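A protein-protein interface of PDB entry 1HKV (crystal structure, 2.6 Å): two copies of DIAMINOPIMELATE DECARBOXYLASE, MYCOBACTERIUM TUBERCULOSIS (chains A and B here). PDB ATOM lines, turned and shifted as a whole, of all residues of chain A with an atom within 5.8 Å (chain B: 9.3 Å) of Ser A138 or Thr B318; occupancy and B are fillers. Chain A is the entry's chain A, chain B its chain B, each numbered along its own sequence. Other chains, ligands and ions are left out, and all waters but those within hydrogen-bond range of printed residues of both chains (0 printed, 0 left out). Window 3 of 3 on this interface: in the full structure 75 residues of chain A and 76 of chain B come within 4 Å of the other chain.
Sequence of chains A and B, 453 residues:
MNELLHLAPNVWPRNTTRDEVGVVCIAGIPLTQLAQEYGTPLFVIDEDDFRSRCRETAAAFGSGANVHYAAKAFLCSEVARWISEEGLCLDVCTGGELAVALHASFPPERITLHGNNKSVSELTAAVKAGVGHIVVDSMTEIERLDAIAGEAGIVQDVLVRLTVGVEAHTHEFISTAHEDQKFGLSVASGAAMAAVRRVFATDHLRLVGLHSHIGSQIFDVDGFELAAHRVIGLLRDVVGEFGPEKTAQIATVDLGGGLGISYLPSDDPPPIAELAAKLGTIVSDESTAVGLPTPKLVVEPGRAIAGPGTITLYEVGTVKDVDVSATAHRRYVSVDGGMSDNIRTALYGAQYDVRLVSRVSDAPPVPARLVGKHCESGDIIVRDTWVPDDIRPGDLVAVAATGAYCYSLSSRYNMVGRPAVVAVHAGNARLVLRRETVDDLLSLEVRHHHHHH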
ATOM      1  N   ASN A 116     -24.004  -1.156 -32.980  1.00  0.00           N
ATOM      2  CA  ASN A 116     -22.958  -0.987 -31.995  1.00  0.00           C
ATOM      3  C   ASN A 116     -23.399  -1.013 -30.545  1.00  0.00           C
ATOM      4  O   ASN A 116     -22.532  -0.932 -29.629  1.00  0.00           O
ATOM      5  CB  ASN A 116     -22.238   0.355 -32.219  1.00  0.00           C
ATOM      6  CG  ASN A 116     -23.134   1.535 -32.015  1.00  0.00           C
ATOM      7  OD1 ASN A 116     -23.196   2.158 -30.889  1.00  0.00           O
ATOM      8  ND2 ASN A 116     -23.866   1.891 -33.089  1.00  0.00           N
ATOM      9  N   ASN A 117     -24.715  -1.016 -30.295  1.00  0.00           N
ATOM     10  CA  ASN A 117     -25.216  -0.963 -28.892  1.00  0.00           C
ATOM     11  C   ASN A 117     -26.472  -1.698 -28.693  1.00  0.00           C
ATOM     12  O   ASN A 117     -27.437  -1.154 -28.108  1.00  0.00           O
ATOM     13  CB  ASN A 117     -25.447   0.442 -28.469  1.00  0.00           C
ATOM     14  CG  ASN A 117     -25.649   0.587 -26.934  1.00  0.00           C
ATOM     15  OD1 ASN A 117     -26.253   1.611 -26.467  1.00  0.00           O
ATOM     16  ND2 ASN A 117     -25.123  -0.415 -26.122  1.00  0.00           N
ATOM     17  N   LYS A 118     -26.485  -2.927 -29.177  1.00  0.00           N
ATOM     18  CA  LYS A 118     -27.668  -3.773 -29.096  1.00  0.00           C
ATOM     19  C   LYS A 118     -28.004  -3.995 -27.635  1.00  0.00           C
ATOM     20  O   LYS A 118     -27.130  -4.344 -26.820  1.00  0.00           O
ATOM     21  CB  LYS A 118     -27.443  -5.111 -29.804  1.00  0.00           C
ATOM     22  CG  LYS A 118     -27.004  -4.995 -31.285  1.00  0.00           C
ATOM     23  CD  LYS A 118     -27.100  -6.346 -31.958  1.00  0.00           C
ATOM     24  CE  LYS A 118     -26.502  -6.378 -33.375  1.00  0.00           C
ATOM     25  NZ  LYS A 118     -24.997  -6.000 -33.453  1.00  0.00           N
ATOM     26  N   VAL A 136     -21.984  -9.145 -34.704  1.00  0.00           N
ATOM     27  CA  VAL A 136     -21.585  -8.721 -33.378  1.00  0.00           C
ATOM     28  C   VAL A 136     -20.535  -7.683 -33.515  1.00  0.00           C
ATOM     29  O   VAL A 136     -19.749  -7.703 -34.460  1.00  0.00           O
ATOM     30  CB  VAL A 136     -20.940  -9.938 -32.540  1.00  0.00           C
ATOM     31  CG1 VAL A 136     -21.948 -10.975 -32.231  1.00  0.00           C
ATOM     32  CG2 VAL A 136     -19.723 -10.554 -33.326  1.00  0.00           C
ATOM     33  N   ASP A 137     -20.491  -6.803 -32.531  1.00  0.00           N
ATOM     34  CA  ASP A 137     -19.696  -5.528 -32.613  1.00  0.00           C
ATOM     35  C   ASP A 137     -18.844  -5.226 -31.367  1.00  0.00           C
ATOM     36  O   ASP A 137     -18.113  -4.254 -31.353  1.00  0.00           O
ATOM     37  CB  ASP A 137     -20.657  -4.322 -32.851  1.00  0.00           C
ATOM     38  CG  ASP A 137     -20.000  -3.211 -33.552  1.00  0.00           C
ATOM     39  OD1 ASP A 137     -19.706  -3.402 -34.793  1.00  0.00           O
ATOM     40  OD2 ASP A 137     -19.714  -2.109 -32.963  1.00  0.00           O
ATOM     41  N   SER A 138     -18.999  -6.037 -30.325  1.00  0.00           N
ATOM     42  CA  SER A 138     -18.253  -5.882 -29.047  1.00  0.00           C
ATOM     43  C   SER A 138     -18.122  -7.208 -28.245  1.00  0.00           C
ATOM     44  O   SER A 138     -18.903  -8.126 -28.412  1.00  0.00           O
ATOM     45  CB  SER A 138     -18.912  -4.862 -28.176  1.00  0.00           C
ATOM     46  OG  SER A 138     -20.194  -5.311 -27.780  1.00  0.00           O
ATOM     47  N   MET A 139     -17.101  -7.292 -27.410  1.00  0.00           N
ATOM     48  CA  MET A 139     -16.991  -8.389 -26.437  1.00  0.00           C
ATOM     49  C   MET A 139     -18.296  -8.464 -25.576  1.00  0.00           C
ATOM     50  O   MET A 139     -18.822  -9.557 -25.292  1.00  0.00           O
ATOM     51  CB  MET A 139     -15.751  -8.191 -25.511  1.00  0.00           C
ATOM     52  CG  MET A 139     -14.374  -8.411 -26.167  1.00  0.00           C
ATOM     53  SD  MET A 139     -14.215  -9.991 -27.126  1.00  0.00           S
ATOM     54  CE  MET A 139     -13.226  -9.435 -28.405  1.00  0.00           C
ATOM     55  N   THR A 140     -18.813  -7.323 -25.166  1.00  0.00           N
ATOM     56  CA  THR A 140     -19.988  -7.338 -24.309  1.00  0.00           C
ATOM     57  C   THR A 140     -21.224  -7.962 -25.054  1.00  0.00           C
ATOM     58  O   THR A 140     -21.996  -8.708 -24.482  1.00  0.00           O
ATOM     59  CB  THR A 140     -20.319  -5.942 -23.853  1.00  0.00           C
ATOM     60  OG1 THR A 140     -19.130  -5.254 -23.423  1.00  0.00           O
ATOM     61  CG2 THR A 140     -21.154  -5.982 -22.595  1.00  0.00           C
ATOM     62  N   GLU A 141     -21.372  -7.651 -26.331  1.00  0.00           N
ATOM     63  CA  GLU A 141     -22.499  -8.138 -27.076  1.00  0.00           C
ATOM     64  C   GLU A 141     -22.331  -9.627 -27.230  1.00  0.00           C
ATOM     65  O   GLU A 141     -23.283 -10.338 -27.201  1.00  0.00           O
ATOM     66  CB  GLU A 141     -22.630  -7.423 -28.458  1.00  0.00           C
ATOM     67  CG  GLU A 141     -23.864  -7.821 -29.250  1.00  0.00           C
ATOM     68  CD  GLU A 141     -23.736  -7.565 -30.748  1.00  0.00           C
ATOM     69  OE1 GLU A 141     -23.245  -6.435 -31.138  1.00  0.00           O
ATOM     70  OE2 GLU A 141     -24.146  -8.485 -31.545  1.00  0.00           O
ATOM     71  N   ILE A 142     -21.095 -10.095 -27.384  1.00  0.00           N
ATOM     72  CA  ILE A 142     -20.848 -11.536 -27.576  1.00  0.00           C
ATOM     73  C   ILE A 142     -21.238 -12.351 -26.295  1.00  0.00           C
ATOM     74  O   ILE A 142     -21.817 -13.410 -26.384  1.00  0.00           O
ATOM     75  CB  ILE A 142     -19.391 -11.801 -27.959  1.00  0.00           C
ATOM     76  CG1 ILE A 142     -19.072 -11.167 -29.285  1.00  0.00           C
ATOM     77  CG2 ILE A 142     -19.117 -13.362 -28.123  1.00  0.00           C
ATOM     78  CD1 ILE A 142     -17.585 -11.069 -29.579  1.00  0.00           C
ATOM     79  N   GLU A 143     -20.917 -11.803 -25.139  1.00  0.00           N
ATOM     80  CA  GLU A 143     -21.286 -12.386 -23.897  1.00  0.00           C
ATOM     81  C   GLU A 143     -22.780 -12.452 -23.758  1.00  0.00           C
ATOM     82  O   GLU A 143     -23.322 -13.499 -23.406  1.00  0.00           O
ATOM     83  CB  GLU A 143     -20.734 -11.571 -22.754  1.00  0.00           C
ATOM     84  CG  GLU A 143     -19.562 -12.210 -22.082  1.00  0.00           C
ATOM     85  CD  GLU A 143     -18.248 -11.529 -22.449  1.00  0.00           C
ATOM     86  OE1 GLU A 143     -18.076 -10.295 -22.077  1.00  0.00           O
ATOM     87  OE2 GLU A 143     -17.363 -12.220 -23.095  1.00  0.00           O
ATOM     88  N   ARG A 144     -23.455 -11.338 -24.029  1.00  0.00           N
ATOM     89  CA  ARG A 144     -24.909 -11.293 -23.942  1.00  0.00           C
ATOM     90  C   ARG A 144     -25.560 -12.246 -24.922  1.00  0.00           C
ATOM     91  O   ARG A 144     -26.467 -12.994 -24.564  1.00  0.00           O
ATOM     92  CB  ARG A 144     -25.413  -9.900 -24.214  1.00  0.00           C
ATOM     93  CG  ARG A 144     -25.037  -8.891 -23.198  1.00  0.00           C
ATOM     94  CD  ARG A 144     -25.050  -7.450 -23.778  1.00  0.00           C
ATOM     95  NE  ARG A 144     -25.031  -6.461 -22.708  1.00  0.00           N
ATOM     96  CZ  ARG A 144     -24.811  -5.187 -22.883  1.00  0.00           C
ATOM     97  NH1 ARG A 144     -24.805  -4.378 -21.838  1.00  0.00           N
ATOM     98  NH2 ARG A 144     -24.587  -4.709 -24.108  1.00  0.00           N
ATOM     99  N   LEU A 185     -14.264  -4.261 -34.561  1.00  0.00           N
ATOM    100  CA  LEU A 185     -13.123  -4.646 -33.778  1.00  0.00           C
ATOM    101  C   LEU A 185     -11.892  -4.606 -34.664  1.00  0.00           C
ATOM    102  O   LEU A 185     -11.922  -5.086 -35.800  1.00  0.00           O
ATOM    103  CB  LEU A 185     -13.332  -6.057 -33.221  1.00  0.00           C
ATOM    104  CG  LEU A 185     -14.469  -6.095 -32.151  1.00  0.00           C
ATOM    105  CD1 LEU A 185     -15.000  -7.496 -31.972  1.00  0.00           C
ATOM    106  CD2 LEU A 185     -14.028  -5.518 -30.785  1.00  0.00           C
ATOM    107  N   GLU B 315     -28.763   5.705 -20.538  1.00  0.00           N
ATOM    108  CA  GLU B 315     -28.151   4.515 -20.001  1.00  0.00           C
ATOM    109  C   GLU B 315     -27.027   3.957 -20.904  1.00  0.00           C
ATOM    110  O   GLU B 315     -27.239   3.530 -22.029  1.00  0.00           O
ATOM    111  CB  GLU B 315     -29.201   3.442 -19.811  1.00  0.00           C
ATOM    112  CG  GLU B 315     -28.751   2.276 -18.914  1.00  0.00           C
ATOM    113  CD  GLU B 315     -29.797   1.157 -18.838  1.00  0.00           C
ATOM    114  OE1 GLU B 315     -30.937   1.455 -18.433  1.00  0.00           O
ATOM    115  OE2 GLU B 315     -29.487   0.004 -19.195  1.00  0.00           O
ATOM    116  N   VAL B 316     -25.844   3.909 -20.353  1.00  0.00           N
ATOM    117  CA  VAL B 316     -24.745   3.313 -21.023  1.00  0.00           C
ATOM    118  C   VAL B 316     -25.099   1.878 -21.343  1.00  0.00           C
ATOM    119  O   VAL B 316     -25.574   1.155 -20.485  1.00  0.00           O
ATOM    120  CB  VAL B 316     -23.533   3.335 -20.141  1.00  0.00           C
ATOM    121  CG1 VAL B 316     -22.294   2.832 -20.901  1.00  0.00           C
ATOM    122  CG2 VAL B 316     -23.312   4.798 -19.538  1.00  0.00           C
ATOM    123  N   GLY B 317     -24.890   1.473 -22.579  1.00  0.00           N
ATOM    124  CA  GLY B 317     -25.166   0.116 -22.984  1.00  0.00           C
ATOM    125  C   GLY B 317     -23.907  -0.640 -23.308  1.00  0.00           C
ATOM    126  O   GLY B 317     -23.814  -1.850 -23.017  1.00  0.00           O
ATOM    127  N   THR B 318     -22.921   0.044 -23.931  1.00  0.00           N
ATOM    128  CA  THR B 318     -21.676  -0.624 -24.357  1.00  0.00           C
ATOM    129  C   THR B 318     -20.516   0.287 -24.100  1.00  0.00           C
ATOM    130  O   THR B 318     -20.657   1.496 -24.151  1.00  0.00           O
ATOM    131  CB  THR B 318     -21.707  -1.020 -25.847  1.00  0.00           C
ATOM    132  OG1 THR B 318     -22.891  -1.740 -26.143  1.00  0.00           O
ATOM    133  CG2 THR B 318     -20.638  -2.074 -26.186  1.00  0.00           C
ATOM    134  N   VAL B 319     -19.365  -0.310 -23.768  1.00  0.00           N
ATOM    135  CA  VAL B 319     -18.181   0.415 -23.540  1.00  0.00           C
ATOM    136  C   VAL B 319     -17.091  -0.301 -24.298  1.00  0.00           C
ATOM    137  O   VAL B 319     -16.726  -1.429 -23.970  1.00  0.00           O
ATOM    138  CB  VAL B 319     -17.840   0.530 -22.034  1.00  0.00           C
ATOM    139  CG1 VAL B 319     -16.487   1.238 -21.815  1.00  0.00           C
ATOM    140  CG2 VAL B 319     -18.837   1.316 -21.346  1.00  0.00           C
ATOM    141  N   LYS B 320     -16.553   0.362 -25.317  1.00  0.00           N
ATOM    142  CA  LYS B 320     -15.507  -0.203 -26.143  1.00  0.00           C
ATOM    143  C   LYS B 320     -14.316   0.724 -26.053  1.00  0.00           C
ATOM    144  O   LYS B 320     -14.471   1.983 -25.998  1.00  0.00           O
ATOM    145  CB  LYS B 320     -15.990  -0.341 -27.599  1.00  0.00           C
ATOM    146  CG  LYS B 320     -15.050  -1.045 -28.525  1.00  0.00           C
ATOM    147  CD  LYS B 320     -15.451  -0.871 -30.002  1.00  0.00           C
ATOM    148  CE  LYS B 320     -16.568  -1.817 -30.401  1.00  0.00           C
ATOM    149  NZ  LYS B 320     -16.934  -1.830 -31.896  1.00  0.00           N
ATOM    150  N   ASP B 321     -13.133   0.124 -26.055  1.00  0.00           N
ATOM    151  CA  ASP B 321     -11.891   0.842 -25.928  1.00  0.00           C
ATOM    152  C   ASP B 321     -11.215   0.816 -27.248  1.00  0.00           C
ATOM    153  O   ASP B 321     -10.805  -0.233 -27.689  1.00  0.00           O
ATOM    154  CB  ASP B 321     -11.034   0.121 -24.932  1.00  0.00           C
ATOM    155  CG  ASP B 321     -10.016   1.003 -24.320  1.00  0.00           C
ATOM    156  OD1 ASP B 321      -8.837   0.515 -24.170  1.00  0.00           O
ATOM    157  OD2 ASP B 321     -10.283   2.213 -23.949  1.00  0.00           O
ATOM    158  N   ARG B 331     -12.099   5.981 -25.250  1.00  0.00           N
ATOM    159  CA  ARG B 331     -13.173   5.194 -24.630  1.00  0.00           C
ATOM    160  C   ARG B 331     -14.524   5.491 -25.252  1.00  0.00           C
ATOM    161  O   ARG B 331     -15.141   6.521 -24.951  1.00  0.00           O
ATOM    162  CB  ARG B 331     -13.239   5.488 -23.142  1.00  0.00           C
ATOM    163  CG  ARG B 331     -13.995   4.340 -22.269  1.00  0.00           C
ATOM    164  CD  ARG B 331     -13.405   2.858 -22.424  1.00  0.00           C
ATOM    165  NE  ARG B 331     -12.017   2.724 -22.008  1.00  0.00           N
ATOM    166  CZ  ARG B 331     -11.597   2.856 -20.760  1.00  0.00           C
ATOM    167  NH1 ARG B 331     -10.343   2.731 -20.491  1.00  0.00           N
ATOM    168  NH2 ARG B 331     -12.416   3.138 -19.797  1.00  0.00           N
ATOM    169  N   TYR B 332     -14.972   4.614 -26.148  1.00  0.00           N
ATOM    170  CA  TYR B 332     -16.267   4.796 -26.810  1.00  0.00           C
ATOM    171  C   TYR B 332     -17.390   4.303 -25.906  1.00  0.00           C
ATOM    172  O   TYR B 332     -17.564   3.092 -25.691  1.00  0.00           O
ATOM    173  CB  TYR B 332     -16.320   4.083 -28.194  1.00  0.00           C
ATOM    174  CG  TYR B 332     -15.790   4.940 -29.312  1.00  0.00           C
ATOM    175  CD1 TYR B 332     -14.436   5.099 -29.485  1.00  0.00           C
ATOM    176  CD2 TYR B 332     -16.654   5.640 -30.182  1.00  0.00           C
ATOM    177  CE1 TYR B 332     -13.913   5.912 -30.524  1.00  0.00           C
ATOM    178  CE2 TYR B 332     -16.125   6.476 -31.233  1.00  0.00           C
ATOM    179  CZ  TYR B 332     -14.745   6.595 -31.367  1.00  0.00           C
ATOM    180  OH  TYR B 332     -14.152   7.351 -32.327  1.00  0.00           O
ATOM    181  N   VAL B 333     -18.153   5.245 -25.357  1.00  0.00           N
ATOM    182  CA  VAL B 333     -19.247   4.846 -24.545  1.00  0.00           C
ATOM    183  C   VAL B 333     -20.606   5.056 -25.255  1.00  0.00           C
ATOM    184  O   VAL B 333     -21.099   6.151 -25.381  1.00  0.00           O
ATOM    185  CB  VAL B 333     -19.132   5.375 -23.061  1.00  0.00           C
ATOM    186  CG1 VAL B 333     -18.011   6.282 -22.900  1.00  0.00           C
ATOM    187  CG2 VAL B 333     -20.430   5.978 -22.550  1.00  0.00           C
ATOM    188  N   SER B 334     -21.152   3.920 -25.719  1.00  0.00           N
ATOM    189  CA  SER B 334     -22.382   3.842 -26.486  1.00  0.00           C
ATOM    190  C   SER B 334     -23.585   3.828 -25.594  1.00  0.00           C
ATOM    191  O   SER B 334     -23.604   3.192 -24.545  1.00  0.00           O
ATOM    192  CB  SER B 334     -22.395   2.581 -27.371  1.00  0.00           C
ATOM    193  OG  SER B 334     -21.033   2.103 -27.623  1.00  0.00           O
ATOM    194  N   VAL B 335     -24.626   4.524 -26.031  1.00  0.00           N
ATOM    195  CA  VAL B 335     -25.642   4.932 -25.140  1.00  0.00           C
ATOM    196  C   VAL B 335     -27.016   4.734 -25.742  1.00  0.00           C
ATOM    197  O   VAL B 335     -27.228   4.159 -26.823  1.00  0.00           O
ATOM    198  CB  VAL B 335     -25.363   6.364 -24.719  1.00  0.00           C
ATOM    199  CG1 VAL B 335     -25.977   7.354 -25.692  1.00  0.00           C
ATOM    200  CG2 VAL B 335     -25.765   6.612 -23.312  1.00  0.00           C
ATOM    201  N   ASP B 336     -27.937   5.166 -24.995  1.00  0.00           N
ATOM    202  CA  ASP B 336     -29.297   4.746 -25.066  1.00  0.00           C
ATOM    203  C   ASP B 336     -30.136   5.272 -26.384  1.00  0.00           C
ATOM    204  O   ASP B 336     -30.982   4.560 -26.947  1.00  0.00           O
ATOM    205  CB  ASP B 336     -29.924   5.294 -23.727  1.00  0.00           C
ATOM    206  CG  ASP B 336     -30.925   4.477 -23.254  1.00  0.00           C
ATOM    207  OD1 ASP B 336     -31.496   4.748 -22.182  1.00  0.00           O
ATOM    208  OD2 ASP B 336     -31.282   3.505 -23.922  1.00  0.00           O
ATOM    209  N   ARG B 369     -15.646   9.381 -26.122  1.00  0.00           N
ATOM    210  CA  ARG B 369     -16.650   9.796 -27.086  1.00  0.00           C
ATOM    211  C   ARG B 369     -17.981   9.153 -26.713  1.00  0.00           C
ATOM    212  O   ARG B 369     -18.121   7.951 -26.785  1.00  0.00           O
ATOM    213  CB  ARG B 369     -16.258   9.267 -28.482  1.00  0.00           C
ATOM    214  CG  ARG B 369     -15.616  10.306 -29.390  1.00  0.00           C
ATOM    215  CD  ARG B 369     -16.198  10.459 -30.712  1.00  0.00           C
ATOM    216  NE  ARG B 369     -15.190  10.395 -31.796  1.00  0.00           N
ATOM    217  CZ  ARG B 369     -14.104  11.188 -31.916  1.00  0.00           C
ATOM    218  NH1 ARG B 369     -13.793  12.100 -31.027  1.00  0.00           N
ATOM    219  NH2 ARG B 369     -13.321  11.025 -32.941  1.00  0.00           N
ATOM    220  N   LEU B 370     -18.942   9.967 -26.299  1.00  0.00           N
ATOM    221  CA  LEU B 370     -20.313   9.505 -26.083  1.00  0.00           C
ATOM    222  C   LEU B 370     -21.002   9.379 -27.400  1.00  0.00           C
ATOM    223  O   LEU B 370     -21.159  10.352 -28.135  1.00  0.00           O
ATOM    224  CB  LEU B 370     -21.054  10.461 -25.206  1.00  0.00           C
ATOM    225  CG  LEU B 370     -22.386   9.998 -24.720  1.00  0.00           C
ATOM    226  CD1 LEU B 370     -22.149   9.108 -23.551  1.00  0.00           C
ATOM    227  CD2 LEU B 370     -23.313  11.225 -24.338  1.00  0.00           C
ATOM    228  N   VAL B 371     -21.403   8.166 -27.690  1.00  0.00           N
ATOM    229  CA  VAL B 371     -21.798   7.763 -28.981  1.00  0.00           C
ATOM    230  C   VAL B 371     -23.212   7.163 -28.859  1.00  0.00           C
ATOM    231  O   VAL B 371     -23.682   6.913 -27.760  1.00  0.00           O
ATOM    232  CB  VAL B 371     -20.701   6.799 -29.521  1.00  0.00           C
ATOM    233  CG1 VAL B 371     -21.157   5.330 -29.630  1.00  0.00           C
ATOM    234  CG2 VAL B 371     -20.151   7.278 -30.766  1.00  0.00           C
ATOM    235  N   GLY B 372     -23.920   6.972 -29.959  1.00  0.00           N
ATOM    236  CA  GLY B 372     -25.343   6.614 -29.878  1.00  0.00           C
ATOM    237  C   GLY B 372     -25.507   5.209 -30.338  1.00  0.00           C
ATOM    238  O   GLY B 372     -24.509   4.437 -30.390  1.00  0.00           O
ATOM    239  N   LYS B 373     -26.737   4.826 -30.734  1.00  0.00           N
ATOM    240  CA  LYS B 373     -26.963   3.448 -31.144  1.00  0.00           C
ATOM    241  C   LYS B 373     -27.369   3.213 -32.645  1.00  0.00           C
ATOM    242  O   LYS B 373     -27.664   2.086 -33.044  1.00  0.00           O
ATOM    243  CB  LYS B 373     -27.962   2.813 -30.214  1.00  0.00           C
ATOM    244  CG  LYS B 373     -29.346   3.536 -30.149  1.00  0.00           C
ATOM    245  CD  LYS B 373     -30.448   2.690 -29.443  1.00  0.00           C
ATOM    246  CE  LYS B 373     -30.713   1.289 -30.149  1.00  0.00           C
ATOM    247  NZ  LYS B 373     -31.513   0.294 -29.203  1.00  0.00           N
ATOM    248  N   VAL B 387     -14.551  10.402 -19.280  1.00  0.00           N
ATOM    249  CA  VAL B 387     -15.336   9.601 -18.385  1.00  0.00           C
ATOM    250  C   VAL B 387     -14.490   8.809 -17.343  1.00  0.00           C
ATOM    251  O   VAL B 387     -13.367   8.336 -17.635  1.00  0.00           O
ATOM    252  CB  VAL B 387     -16.154   8.645 -19.132  1.00  0.00           C
ATOM    253  CG1 VAL B 387     -17.151   9.397 -19.947  1.00  0.00           C
ATOM    254  CG2 VAL B 387     -15.302   7.742 -19.981  1.00  0.00           C
ATOM    255  N   ILE B 391     -16.319   3.267 -15.886  1.00  0.00           N
ATOM    256  CA  ILE B 391     -17.627   3.433 -16.582  1.00  0.00           C
ATOM    257  C   ILE B 391     -18.041   2.160 -17.194  1.00  0.00           C
ATOM    258  O   ILE B 391     -17.249   1.497 -17.799  1.00  0.00           O
ATOM    259  CB  ILE B 391     -17.529   4.502 -17.691  1.00  0.00           C
ATOM    260  CG1 ILE B 391     -18.902   4.731 -18.394  1.00  0.00           C
ATOM    261  CG2 ILE B 391     -16.507   4.113 -18.712  1.00  0.00           C
ATOM    262  CD1 ILE B 391     -19.776   5.760 -17.733  1.00  0.00           C
ATOM    263  N   ARG B 392     -19.305   1.795 -17.014  1.00  0.00           N
ATOM    264  CA  ARG B 392     -19.762   0.455 -17.360  1.00  0.00           C
ATOM    265  C   ARG B 392     -21.242   0.442 -17.589  1.00  0.00           C
ATOM    266  O   ARG B 392     -21.946   1.371 -17.153  1.00  0.00           O
ATOM    267  CB  ARG B 392     -19.316  -0.560 -16.284  1.00  0.00           C
ATOM    268  CG  ARG B 392     -20.411  -1.152 -15.277  1.00  0.00           C
ATOM    269  CD  ARG B 392     -20.774  -0.247 -14.009  1.00  0.00           C
ATOM    270  NE  ARG B 392     -19.804  -0.318 -12.904  1.00  0.00           N
ATOM    271  CZ  ARG B 392     -20.048   0.112 -11.639  1.00  0.00           C
ATOM    272  NH1 ARG B 392     -19.108   0.035 -10.733  1.00  0.00           N
ATOM    273  NH2 ARG B 392     -21.229   0.617 -11.300  1.00  0.00           N
ATOM    274  N   PRO B 393     -21.717  -0.557 -18.338  1.00  0.00           N
ATOM    275  CA  PRO B 393     -23.130  -0.615 -18.745  1.00  0.00           C
ATOM    276  C   PRO B 393     -24.004  -0.573 -17.592  1.00  0.00           C
ATOM    277  O   PRO B 393     -23.537  -0.920 -16.539  1.00  0.00           O
ATOM    278  CB  PRO B 393     -23.248  -1.978 -19.472  1.00  0.00           C
ATOM    279  CG  PRO B 393     -21.839  -2.300 -19.928  1.00  0.00           C
ATOM    280  CD  PRO B 393     -20.942  -1.678 -18.891  1.00  0.00           C
ATOM    281  N   GLY B 394     -25.256  -0.128 -17.769  1.00  0.00           N
ATOM    282  CA  GLY B 394     -26.180   0.126 -16.666  1.00  0.00           C
ATOM    283  C   GLY B 394     -25.934   1.417 -15.893  1.00  0.00           C
ATOM    284  O   GLY B 394     -26.827   1.864 -15.167  1.00  0.00           O
ATOM    285  N   ASP B 395     -24.753   2.044 -16.033  1.00  0.00           N
ATOM    286  CA  ASP B 395     -24.566   3.432 -15.548  1.00  0.00           C
ATOM    287  C   ASP B 395     -25.546   4.459 -16.208  1.00  0.00           C
ATOM    288  O   ASP B 395     -25.982   4.290 -17.367  1.00  0.00           O
ATOM    289  CB  ASP B 395     -23.162   3.907 -15.824  1.00  0.00           C
ATOM    290  CG  ASP B 395     -22.148   3.326 -14.892  1.00  0.00           C
ATOM    291  OD1 ASP B 395     -22.411   3.287 -13.639  1.00  0.00           O
ATOM    292  OD2 ASP B 395     -21.019   2.900 -15.323  1.00  0.00           O
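OD1 of Asn A116 sits close to O of Gly B372, at 2.7 Å. ND2 of Asn A117 is in hydrogen-bond range of OG1 of Thr B318 (2.6 Å). O of Val B335 lies close to OD1 of Asn A117, 2.8 Å away. The side-chain amino group (NZ) of Lys B320 lies within salt-bridge range of the side-chain carboxylate (OD2) of Asp A137 (3.0 Å). The backbone carbonyl oxygen of Gly B317 is in hydrogen-bond range of the guanidinium group of Arg A144, 3.0 Å away.
N of Asp A137 sits at hydrogen-bond distance from OE1 of Glu A141 (3.1 Å). N of Glu A141 is in hydrogen-bond range of OG of Ser A138 (3.0 Å). The backbone carbonyl oxygen (O) of Ser B334 sits at hydrogen-bond distance from the backbone NH (N) of Gly B317. The backbone carbonyl oxygen of Thr B318 lies within hydrogen-bond range of the backbone NH of Ser B334 (2.9 Å). The backbone carbonyl oxygen (O) of Lys B320 lies within hydrogen-bond range of the backbone NH (N) of Tyr B332. The backbone NH (N) of Val B335 lies within hydrogen-bond range of the backbone carbonyl oxygen (O) of Val B371, at 3.1 Å.
Thr B318 touches Asn A116 (OG1 to O, 3.6 Å). Asn A116 touches Ser B334 (OD1 to CB, 3.6 Å). CG1 of Val B371 touches OD1 of Asn A116 (3.98 Å). ND2 of Asn A116 touches C of Lys B373 (3.8 Å). Gly B317 touches Asn A117. OD1 of Asn A117 touches C of Ser B334, at 3.6 Å. CB of Lys B373 touches CB of Asn A117, at 3.9 Å. Ser A138 touches Thr B318. Thr B318 touches Arg A144. CB of Pro B393 touches NH1 of Arg A144, at 3.7 Å.
Ser A138 touches just one residue of chain B: Thr B318. Thr B318 touches four residues of chain A. Asn A117 touches five residues of chain B. Of the printed residues of chain B, Asn A116 touches Thr B318 (3.6 Å), Ser B334 (3.6 Å), Val B371 (3.98 Å), Gly B372 (2.7 Å) and Lys B373 (3.8 Å). Printed residues of chain A within 4 Å of Gly B317: Asn A117 (3.1 Å) and Arg A144 (3.0 Å). Of the printed residues of chain A, Gly B372 touches Asn A116. Printed residues of chain B within 4 Å of Arg A144: Gly B317, Thr B318 and Pro B393. Ile A142 touches none of the printed residues of chain B. The nearest residue of chain B that does not touch Ser A138 is Lys B320 (4.4 Å). The nearest residue of chain A that does not touch Thr B318 is Thr A140 (4.5 Å). The nearest printed residue of chain A that does not touch Pro B393 is Thr A140 (4.6 Å).
Of the 13 printed residues of chain A, 5 touch a printed residue of chain B. Along chain A the printed residues that touch a printed residue of chain B span positions 116 to 144. Printed residues of chain B that touch a printed residue of chain A: Gly B317, Thr B318, Lys B320, Ser B334, Val B335, Val B371, Gly B372, Lys B373 and Pro B393. Hydrophobic or aromatic side chains of chain B that line the printed part of chain A: Val B371 and Pro B393.
No position is printed for both chains.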
